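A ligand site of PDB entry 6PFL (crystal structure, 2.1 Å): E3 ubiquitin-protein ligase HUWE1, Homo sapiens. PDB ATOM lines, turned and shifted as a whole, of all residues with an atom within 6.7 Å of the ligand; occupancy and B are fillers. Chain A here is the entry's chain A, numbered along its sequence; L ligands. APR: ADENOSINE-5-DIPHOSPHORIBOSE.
Residues that only touch the ligand: Trp 10 (3.4 Å), Tyr 21 (3.6 Å), Ala 44 (3.9 Å) and Arg 47 (3.96 Å).
The side-chain hydroxyl of Tyr 49 is in hydrogen-bond range of an oxygen (O2A) of the ligand (2.6 Å). The side-chain hydroxyl of Thr 63 lies within hydrogen-bond range of an oxygen (O2B) of the ligand. NE of Arg 67 is in salt-bridge range of O1A of the ligand, 2.7 Å away. An oxygen (O1B) of the ligand sits at hydrogen-bond distance from the side-chain amide nitrogen (ND2) of Asn 65 (2.8 Å). A nitrogen (N7) of the ligand is in hydrogen-bond range of the side-chain amide nitrogen (NE2) of Gln 58, at 3.0 Å. The side-chain amide nitrogen (ND2) of Asn 60 is in hydrogen-bond range of an oxygen (O2A) of the ligand, 3.0 Å away.
N of Tyr 49 lies within hydrogen-bond range of O of Phe 42, at 3.0 Å. OG1 of Thr 63 sits at hydrogen-bond distance from N of Asn 65 (3.1 Å). The side-chain amide oxygen (OD1) of Asn 60 is in hydrogen-bond range of the backbone NH (N) of Thr 63, at 3.0 Å. NH2 of Arg 67 lies close to ND2 of Asn 65 (3.3 Å). The backbone carbonyl oxygen (O) of Arg 67 is in hydrogen-bond range of the backbone NH (N) of Gln 58, 2.7 Å away. O of Asn 65 sits at hydrogen-bond distance from N of Asn 60, at 3.1 Å. OE1 of Gln 58 sits at hydrogen-bond distance from OH of Tyr 21, 2.6 Å away. The side-chain amide oxygen (OD1) of Asn 60 sits at hydrogen-bond distance from the backbone NH (N) of Glu 62 (2.7 Å).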
ATOM      1  N   TRP A  10      20.071 -26.536  26.637  1.00  0.00           N
ATOM      2  CA  TRP A  10      21.532 -26.618  26.810  1.00  0.00           C
ATOM      3  C   TRP A  10      21.814 -27.498  28.037  1.00  0.00           C
ATOM      4  O   TRP A  10      20.981 -27.470  28.958  1.00  0.00           O
ATOM      5  CB  TRP A  10      22.121 -25.195  26.941  1.00  0.00           C
ATOM      6  CG  TRP A  10      21.655 -24.412  28.126  1.00  0.00           C
ATOM      7  CD1 TRP A  10      20.469 -23.735  28.273  1.00  0.00           C
ATOM      8  CD2 TRP A  10      22.370 -24.229  29.369  1.00  0.00           C
ATOM      9  NE1 TRP A  10      20.397 -23.179  29.516  1.00  0.00           N
ATOM     10  CE2 TRP A  10      21.546 -23.464  30.205  1.00  0.00           C
ATOM     11  CE3 TRP A  10      23.596 -24.672  29.851  1.00  0.00           C
ATOM     12  CZ2 TRP A  10      21.928 -23.113  31.500  1.00  0.00           C
ATOM     13  CZ3 TRP A  10      23.980 -24.327  31.131  1.00  0.00           C
ATOM     14  CH2 TRP A  10      23.153 -23.549  31.941  1.00  0.00           C
ATOM     15  N   PHE A  11      22.903 -28.307  28.023  1.00  0.00           N
ATOM     16  CA  PHE A  11      23.291 -29.215  29.156  1.00  0.00           C
ATOM     17  C   PHE A  11      24.163 -28.447  30.149  1.00  0.00           C
ATOM     18  O   PHE A  11      25.176 -27.863  29.775  1.00  0.00           O
ATOM     19  CB  PHE A  11      23.974 -30.495  28.681  1.00  0.00           C
ATOM     20  CG  PHE A  11      24.080 -31.593  29.722  1.00  0.00           C
ATOM     21  CD1 PHE A  11      22.999 -32.397  30.042  1.00  0.00           C
ATOM     22  CD2 PHE A  11      25.262 -31.785  30.446  1.00  0.00           C
ATOM     23  CE1 PHE A  11      23.081 -33.367  31.032  1.00  0.00           C
ATOM     24  CE2 PHE A  11      25.349 -32.744  31.431  1.00  0.00           C
ATOM     25  CZ  PHE A  11      24.268 -33.543  31.723  1.00  0.00           C
ATOM     26  N   ASP A  12      23.776 -28.528  31.417  1.00  0.00           N
ATOM     27  CA  ASP A  12      24.516 -27.933  32.566  1.00  0.00           C
ATOM     28  C   ASP A  12      25.341 -29.048  33.250  1.00  0.00           C
ATOM     29  O   ASP A  12      24.740 -29.950  33.882  1.00  0.00           O
ATOM     30  CB  ASP A  12      23.505 -27.247  33.482  1.00  0.00           C
ATOM     31  CG  ASP A  12      24.056 -26.714  34.800  1.00  0.00           C
ATOM     32  OD1 ASP A  12      25.257 -26.478  34.874  1.00  0.00           O
ATOM     33  OD2 ASP A  12      23.249 -26.557  35.719  1.00  0.00           O
ATOM     34  N   ASP A  13      26.647 -29.039  33.064  1.00  0.00           N
ATOM     35  CA  ASP A  13      27.577 -30.066  33.579  1.00  0.00           C
ATOM     36  C   ASP A  13      27.676 -29.928  35.116  1.00  0.00           C
ATOM     37  O   ASP A  13      27.895 -30.952  35.764  1.00  0.00           O
ATOM     38  CB  ASP A  13      28.939 -29.950  32.927  1.00  0.00           C
ATOM     39  CG  ASP A  13      29.602 -28.606  33.187  1.00  0.00           C
ATOM     40  OD1 ASP A  13      29.025 -27.821  33.981  1.00  0.00           O
ATOM     41  OD2 ASP A  13      30.657 -28.340  32.604  1.00  0.00           O
ATOM     42  N   ARG A  14      27.468 -28.725  35.648  1.00  0.00           N
ATOM     43  CA  ARG A  14      27.481 -28.437  37.111  1.00  0.00           C
ATOM     44  C   ARG A  14      26.419 -29.287  37.802  1.00  0.00           C
ATOM     45  O   ARG A  14      26.754 -29.990  38.755  1.00  0.00           O
ATOM     46  CB  ARG A  14      27.232 -26.940  37.376  1.00  0.00           C
ATOM     47  N   SER A  20      16.152 -25.587  29.973  1.00  0.00           N
ATOM     48  CA  SER A  20      15.438 -24.778  28.950  1.00  0.00           C
ATOM     49  C   SER A  20      16.049 -23.362  28.900  1.00  0.00           C
ATOM     50  O   SER A  20      16.523 -22.888  29.925  1.00  0.00           O
ATOM     51  CB  SER A  20      13.949 -24.724  29.239  1.00  0.00           C
ATOM     52  OG  SER A  20      13.280 -25.881  28.709  1.00  0.00           O
ATOM     53  N   TYR A  21      16.097 -22.758  27.712  1.00  0.00           N
ATOM     54  CA  TYR A  21      16.424 -21.320  27.525  1.00  0.00           C
ATOM     55  C   TYR A  21      15.240 -20.448  27.996  1.00  0.00           C
ATOM     56  O   TYR A  21      14.099 -20.970  28.097  1.00  0.00           O
ATOM     57  CB  TYR A  21      16.740 -21.053  26.052  1.00  0.00           C
ATOM     58  CG  TYR A  21      18.108 -21.515  25.610  1.00  0.00           C
ATOM     59  CD1 TYR A  21      19.216 -20.725  25.781  1.00  0.00           C
ATOM     60  CD2 TYR A  21      18.267 -22.728  24.955  1.00  0.00           C
ATOM     61  CE1 TYR A  21      20.474 -21.137  25.351  1.00  0.00           C
ATOM     62  CE2 TYR A  21      19.506 -23.150  24.502  1.00  0.00           C
ATOM     63  CZ  TYR A  21      20.618 -22.345  24.712  1.00  0.00           C
ATOM     64  OH  TYR A  21      21.843 -22.766  24.303  1.00  0.00           O
ATOM     65  N   ASN A  25      14.917 -16.114  24.291  1.00  0.00           N
ATOM     66  CA  ASN A  25      16.103 -16.803  23.712  1.00  0.00           C
ATOM     67  C   ASN A  25      15.604 -18.002  22.875  1.00  0.00           C
ATOM     68  O   ASN A  25      15.988 -18.099  21.686  1.00  0.00           O
ATOM     69  CB  ASN A  25      17.104 -17.172  24.815  1.00  0.00           C
ATOM     70  CG  ASN A  25      17.935 -15.998  25.293  1.00  0.00           C
ATOM     71  OD1 ASN A  25      18.076 -15.022  24.575  1.00  0.00           O
ATOM     72  ND2 ASN A  25      18.516 -16.107  26.480  1.00  0.00           N
ATOM     73  N   PHE A  42      22.796 -14.429  20.629  1.00  0.00           N
ATOM     74  CA  PHE A  42      21.924 -13.906  21.694  1.00  0.00           C
ATOM     75  C   PHE A  42      22.735 -13.743  22.981  1.00  0.00           C
ATOM     76  O   PHE A  42      23.966 -14.026  22.994  1.00  0.00           O
ATOM     77  CB  PHE A  42      20.748 -14.865  21.914  1.00  0.00           C
ATOM     78  CG  PHE A  42      21.147 -16.250  22.327  1.00  0.00           C
ATOM     79  CD1 PHE A  42      21.354 -16.554  23.662  1.00  0.00           C
ATOM     80  CD2 PHE A  42      21.330 -17.246  21.384  1.00  0.00           C
ATOM     81  CE1 PHE A  42      21.738 -17.823  24.044  1.00  0.00           C
ATOM     82  CE2 PHE A  42      21.681 -18.533  21.771  1.00  0.00           C
ATOM     83  CZ  PHE A  42      21.913 -18.810  23.095  1.00  0.00           C
ATOM     84  N   ALA A  44      22.569 -14.415  27.422  1.00  0.00           N
ATOM     85  CA  ALA A  44      21.964 -15.002  28.640  1.00  0.00           C
ATOM     86  C   ALA A  44      22.969 -14.877  29.813  1.00  0.00           C
ATOM     87  O   ALA A  44      24.207 -14.973  29.569  1.00  0.00           O
ATOM     88  CB  ALA A  44      21.564 -16.443  28.384  1.00  0.00           C
ATOM     89  N   GLY A  45      22.451 -14.677  31.037  1.00  0.00           N
ATOM     90  CA  GLY A  45      23.254 -14.270  32.212  1.00  0.00           C
ATOM     91  C   GLY A  45      24.115 -13.048  31.923  1.00  0.00           C
ATOM     92  O   GLY A  45      25.222 -12.952  32.501  1.00  0.00           O
ATOM     93  N   ARG A  47      25.700 -12.563  29.258  1.00  0.00           N
ATOM     94  CA  ARG A  47      26.861 -13.162  28.544  1.00  0.00           C
ATOM     95  C   ARG A  47      26.477 -13.393  27.074  1.00  0.00           C
ATOM     96  O   ARG A  47      25.301 -13.572  26.800  1.00  0.00           O
ATOM     97  CB  ARG A  47      27.265 -14.490  29.181  1.00  0.00           C
ATOM     98  CG  ARG A  47      28.118 -14.356  30.440  1.00  0.00           C
ATOM     99  CD  ARG A  47      28.763 -15.676  30.798  1.00  0.00           C
ATOM    100  NE  ARG A  47      29.783 -15.559  31.841  1.00  0.00           N
ATOM    101  CZ  ARG A  47      29.529 -15.540  33.142  1.00  0.00           C
ATOM    102  NH1 ARG A  47      28.285 -15.600  33.583  1.00  0.00           N
ATOM    103  NH2 ARG A  47      30.529 -15.437  34.004  1.00  0.00           N
ATOM    104  N   ARG A  48      27.452 -13.367  26.164  1.00  0.00           N
ATOM    105  CA  ARG A  48      27.191 -13.444  24.707  1.00  0.00           C
ATOM    106  C   ARG A  48      27.469 -14.866  24.209  1.00  0.00           C
ATOM    107  O   ARG A  48      28.636 -15.352  24.379  1.00  0.00           O
ATOM    108  CB  ARG A  48      28.029 -12.389  23.969  1.00  0.00           C
ATOM    109  CG  ARG A  48      27.430 -10.993  24.023  1.00  0.00           C
ATOM    110  CD  ARG A  48      28.186 -10.002  23.143  1.00  0.00           C
ATOM    111  N   TYR A  49      26.452 -15.503  23.578  1.00  0.00           N
ATOM    112  CA  TYR A  49      26.509 -16.897  23.035  1.00  0.00           C
ATOM    113  C   TYR A  49      26.151 -16.915  21.548  1.00  0.00           C
ATOM    114  O   TYR A  49      25.246 -16.182  21.100  1.00  0.00           O
ATOM    115  CB  TYR A  49      25.564 -17.840  23.794  1.00  0.00           C
ATOM    116  CG  TYR A  49      25.897 -18.039  25.255  1.00  0.00           C
ATOM    117  CD1 TYR A  49      26.992 -18.791  25.651  1.00  0.00           C
ATOM    118  CD2 TYR A  49      25.119 -17.447  26.249  1.00  0.00           C
ATOM    119  CE1 TYR A  49      27.315 -18.941  26.991  1.00  0.00           C
ATOM    120  CE2 TYR A  49      25.451 -17.565  27.594  1.00  0.00           C
ATOM    121  CZ  TYR A  49      26.559 -18.310  27.961  1.00  0.00           C
ATOM    122  OH  TYR A  49      26.873 -18.450  29.296  1.00  0.00           O
ATOM    123  N   GLN A  58      26.611 -24.595  22.010  1.00  0.00           N
ATOM    124  CA  GLN A  58      26.579 -23.185  22.411  1.00  0.00           C
ATOM    125  C   GLN A  58      28.002 -22.738  22.769  1.00  0.00           C
ATOM    126  O   GLN A  58      28.700 -23.423  23.575  1.00  0.00           O
ATOM    127  CB  GLN A  58      25.576 -23.045  23.535  1.00  0.00           C
ATOM    128  CG  GLN A  58      25.540 -21.684  24.172  1.00  0.00           C
ATOM    129  CD  GLN A  58      24.943 -21.790  25.544  1.00  0.00           C
ATOM    130  OE1 GLN A  58      23.725 -21.770  25.712  1.00  0.00           O
ATOM    131  NE2 GLN A  58      25.827 -21.956  26.533  1.00  0.00           N
ATOM    132  N   VAL A  59      28.461 -21.690  22.093  1.00  0.00           N
ATOM    133  CA  VAL A  59      29.838 -21.112  22.222  1.00  0.00           C
ATOM    134  C   VAL A  59      29.726 -19.842  23.085  1.00  0.00           C
ATOM    135  O   VAL A  59      28.947 -18.928  22.732  1.00  0.00           O
ATOM    136  CB  VAL A  59      30.435 -20.808  20.831  1.00  0.00           C
ATOM    137  CG1 VAL A  59      31.756 -20.046  20.912  1.00  0.00           C
ATOM    138  CG2 VAL A  59      30.618 -22.077  19.981  1.00  0.00           C
ATOM    139  N   ASN A  60      30.438 -19.804  24.205  1.00  0.00           N
ATOM    140  CA  ASN A  60      30.737 -18.540  24.930  1.00  0.00           C
ATOM    141  C   ASN A  60      31.677 -17.732  24.050  1.00  0.00           C
ATOM    142  O   ASN A  60      32.692 -18.309  23.602  1.00  0.00           O
ATOM    143  CB  ASN A  60      31.327 -18.772  26.312  1.00  0.00           C
ATOM    144  CG  ASN A  60      31.609 -17.458  27.025  1.00  0.00           C
ATOM    145  OD1 ASN A  60      32.434 -16.678  26.567  1.00  0.00           O
ATOM    146  ND2 ASN A  60      30.869 -17.189  28.088  1.00  0.00           N
ATOM    147  N   GLU A  62      33.397 -15.002  24.619  1.00  0.00           N
ATOM    148  CA  GLU A  62      34.648 -14.585  25.343  1.00  0.00           C
ATOM    149  C   GLU A  62      35.685 -15.744  25.333  1.00  0.00           C
ATOM    150  O   GLU A  62      36.861 -15.457  25.072  1.00  0.00           O
ATOM    151  CB  GLU A  62      34.317 -14.105  26.769  1.00  0.00           C
ATOM    152  CG  GLU A  62      33.420 -12.887  26.820  1.00  0.00           C
ATOM    153  N   THR A  63      35.281 -16.983  25.668  1.00  0.00           N
ATOM    154  CA  THR A  63      36.187 -18.074  26.168  1.00  0.00           C
ATOM    155  C   THR A  63      36.394 -19.169  25.100  1.00  0.00           C
ATOM    156  O   THR A  63      37.461 -19.857  25.135  1.00  0.00           O
ATOM    157  CB  THR A  63      35.647 -18.656  27.492  1.00  0.00           C
ATOM    158  OG1 THR A  63      34.426 -19.343  27.261  1.00  0.00           O
ATOM    159  CG2 THR A  63      35.412 -17.571  28.529  1.00  0.00           C
ATOM    160  N   GLY A  64      35.434 -19.338  24.183  1.00  0.00           N
ATOM    161  CA  GLY A  64      35.415 -20.486  23.252  1.00  0.00           C
ATOM    162  C   GLY A  64      34.773 -21.713  23.876  1.00  0.00           C
ATOM    163  O   GLY A  64      34.563 -22.678  23.123  1.00  0.00           O
ATOM    164  N   ASN A  65      34.357 -21.637  25.156  1.00  0.00           N
ATOM    165  CA  ASN A  65      33.795 -22.791  25.926  1.00  0.00           C
ATOM    166  C   ASN A  65      32.544 -23.322  25.205  1.00  0.00           C
ATOM    167  O   ASN A  65      31.638 -22.541  24.901  1.00  0.00           O
ATOM    168  CB  ASN A  65      33.460 -22.442  27.388  1.00  0.00           C
ATOM    169  CG  ASN A  65      33.219 -23.691  28.218  1.00  0.00           C
ATOM    170  OD1 ASN A  65      33.916 -24.686  28.023  1.00  0.00           O
ATOM    171  ND2 ASN A  65      32.210 -23.687  29.091  1.00  0.00           N
ATOM    172  N   ARG A  66      32.491 -24.617  24.946  1.00  0.00           N
ATOM    173  CA  ARG A  66      31.418 -25.267  24.144  1.00  0.00           C
ATOM    174  C   ARG A  66      30.517 -26.088  25.085  1.00  0.00           C
ATOM    175  O   ARG A  66      31.066 -26.909  25.803  1.00  0.00           O
ATOM    176  CB  ARG A  66      32.069 -26.112  23.043  1.00  0.00           C
ATOM    177  CG  ARG A  66      32.950 -25.303  22.094  1.00  0.00           C
ATOM    178  CD  ARG A  66      33.941 -26.112  21.274  1.00  0.00           C
ATOM    179  NE  ARG A  66      33.326 -26.951  20.247  1.00  0.00           N
ATOM    180  CZ  ARG A  66      32.878 -26.548  19.044  1.00  0.00           C
ATOM    181  NH1 ARG A  66      32.931 -25.273  18.669  1.00  0.00           N
ATOM    182  NH2 ARG A  66      32.383 -27.446  18.197  1.00  0.00           N
ATOM    183  N   ARG A  67      29.200 -25.805  25.103  1.00  0.00           N
ATOM    184  CA  ARG A  67      28.155 -26.594  25.818  1.00  0.00           C
ATOM    185  C   ARG A  67      27.166 -27.196  24.812  1.00  0.00           C
ATOM    186  O   ARG A  67      26.811 -26.577  23.840  1.00  0.00           O
ATOM    187  CB  ARG A  67      27.442 -25.719  26.853  1.00  0.00           C
ATOM    188  CG  ARG A  67      28.387 -25.231  27.936  1.00  0.00           C
ATOM    189  CD  ARG A  67      27.697 -24.637  29.142  1.00  0.00           C
ATOM    190  NE  ARG A  67      28.727 -24.066  30.005  1.00  0.00           N
ATOM    191  CZ  ARG A  67      29.282 -24.675  31.072  1.00  0.00           C
ATOM    192  NH1 ARG A  67      28.869 -25.865  31.472  1.00  0.00           N
ATOM    193  NH2 ARG A  67      30.247 -24.066  31.757  1.00  0.00           N
HETATM  194  N1  APR L   1      21.965 -19.761  30.371  1.00  0.00           N
HETATM  195  C2  APR L   1      22.374 -19.522  31.626  1.00  0.00           C
HETATM  196  N3  APR L   1      23.567 -19.738  32.195  1.00  0.00           N
HETATM  197  C4  APR L   1      24.413 -20.306  31.317  1.00  0.00           C
HETATM  198  C5  APR L   1      24.129 -20.648  30.006  1.00  0.00           C
HETATM  199  C6  APR L   1      22.846 -20.368  29.514  1.00  0.00           C
HETATM  200  N6  APR L   1      22.473 -20.610  28.250  1.00  0.00           N
HETATM  201  N7  APR L   1      25.237 -21.224  29.404  1.00  0.00           N
HETATM  202  C8  APR L   1      26.164 -21.230  30.345  1.00  0.00           C
HETATM  203  N9  APR L   1      25.705 -20.683  31.529  1.00  0.00           N
HETATM  204  C1' APR L   1      26.488 -20.521  32.730  1.00  0.00           C
HETATM  205  C2' APR L   1      27.255 -21.803  33.047  1.00  0.00           C
HETATM  206  O2' APR L   1      26.500 -22.644  33.893  1.00  0.00           O
HETATM  207  C3' APR L   1      28.552 -21.290  33.677  1.00  0.00           C
HETATM  208  O3' APR L   1      28.500 -21.388  35.102  1.00  0.00           O
HETATM  209  O4' APR L   1      27.453 -19.516  32.496  1.00  0.00           O
HETATM  210  C4' APR L   1      28.677 -19.822  33.208  1.00  0.00           C
HETATM  211  C5' APR L   1      29.885 -19.494  32.351  1.00  0.00           C
HETATM  212  O5' APR L   1      30.201 -20.626  31.503  1.00  0.00           O
HETATM  213  PA  APR L   1      30.234 -20.468  29.880  1.00  0.00           P
HETATM  214  O1A APR L   1      30.093 -21.809  29.237  1.00  0.00           O
HETATM  215  O2A APR L   1      29.305 -19.369  29.490  1.00  0.00           O
HETATM  216  O3A APR L   1      31.761 -20.018  29.697  1.00  0.00           O
HETATM  217  PB  APR L   1      33.044 -20.483  30.568  1.00  0.00           P
HETATM  218  O1B APR L   1      32.780 -21.857  31.121  1.00  0.00           O
HETATM  219  O2B APR L   1      34.257 -20.267  29.707  1.00  0.00           O
HETATM  220  O5D APR L   1      32.980 -19.424  31.761  1.00  0.00           O
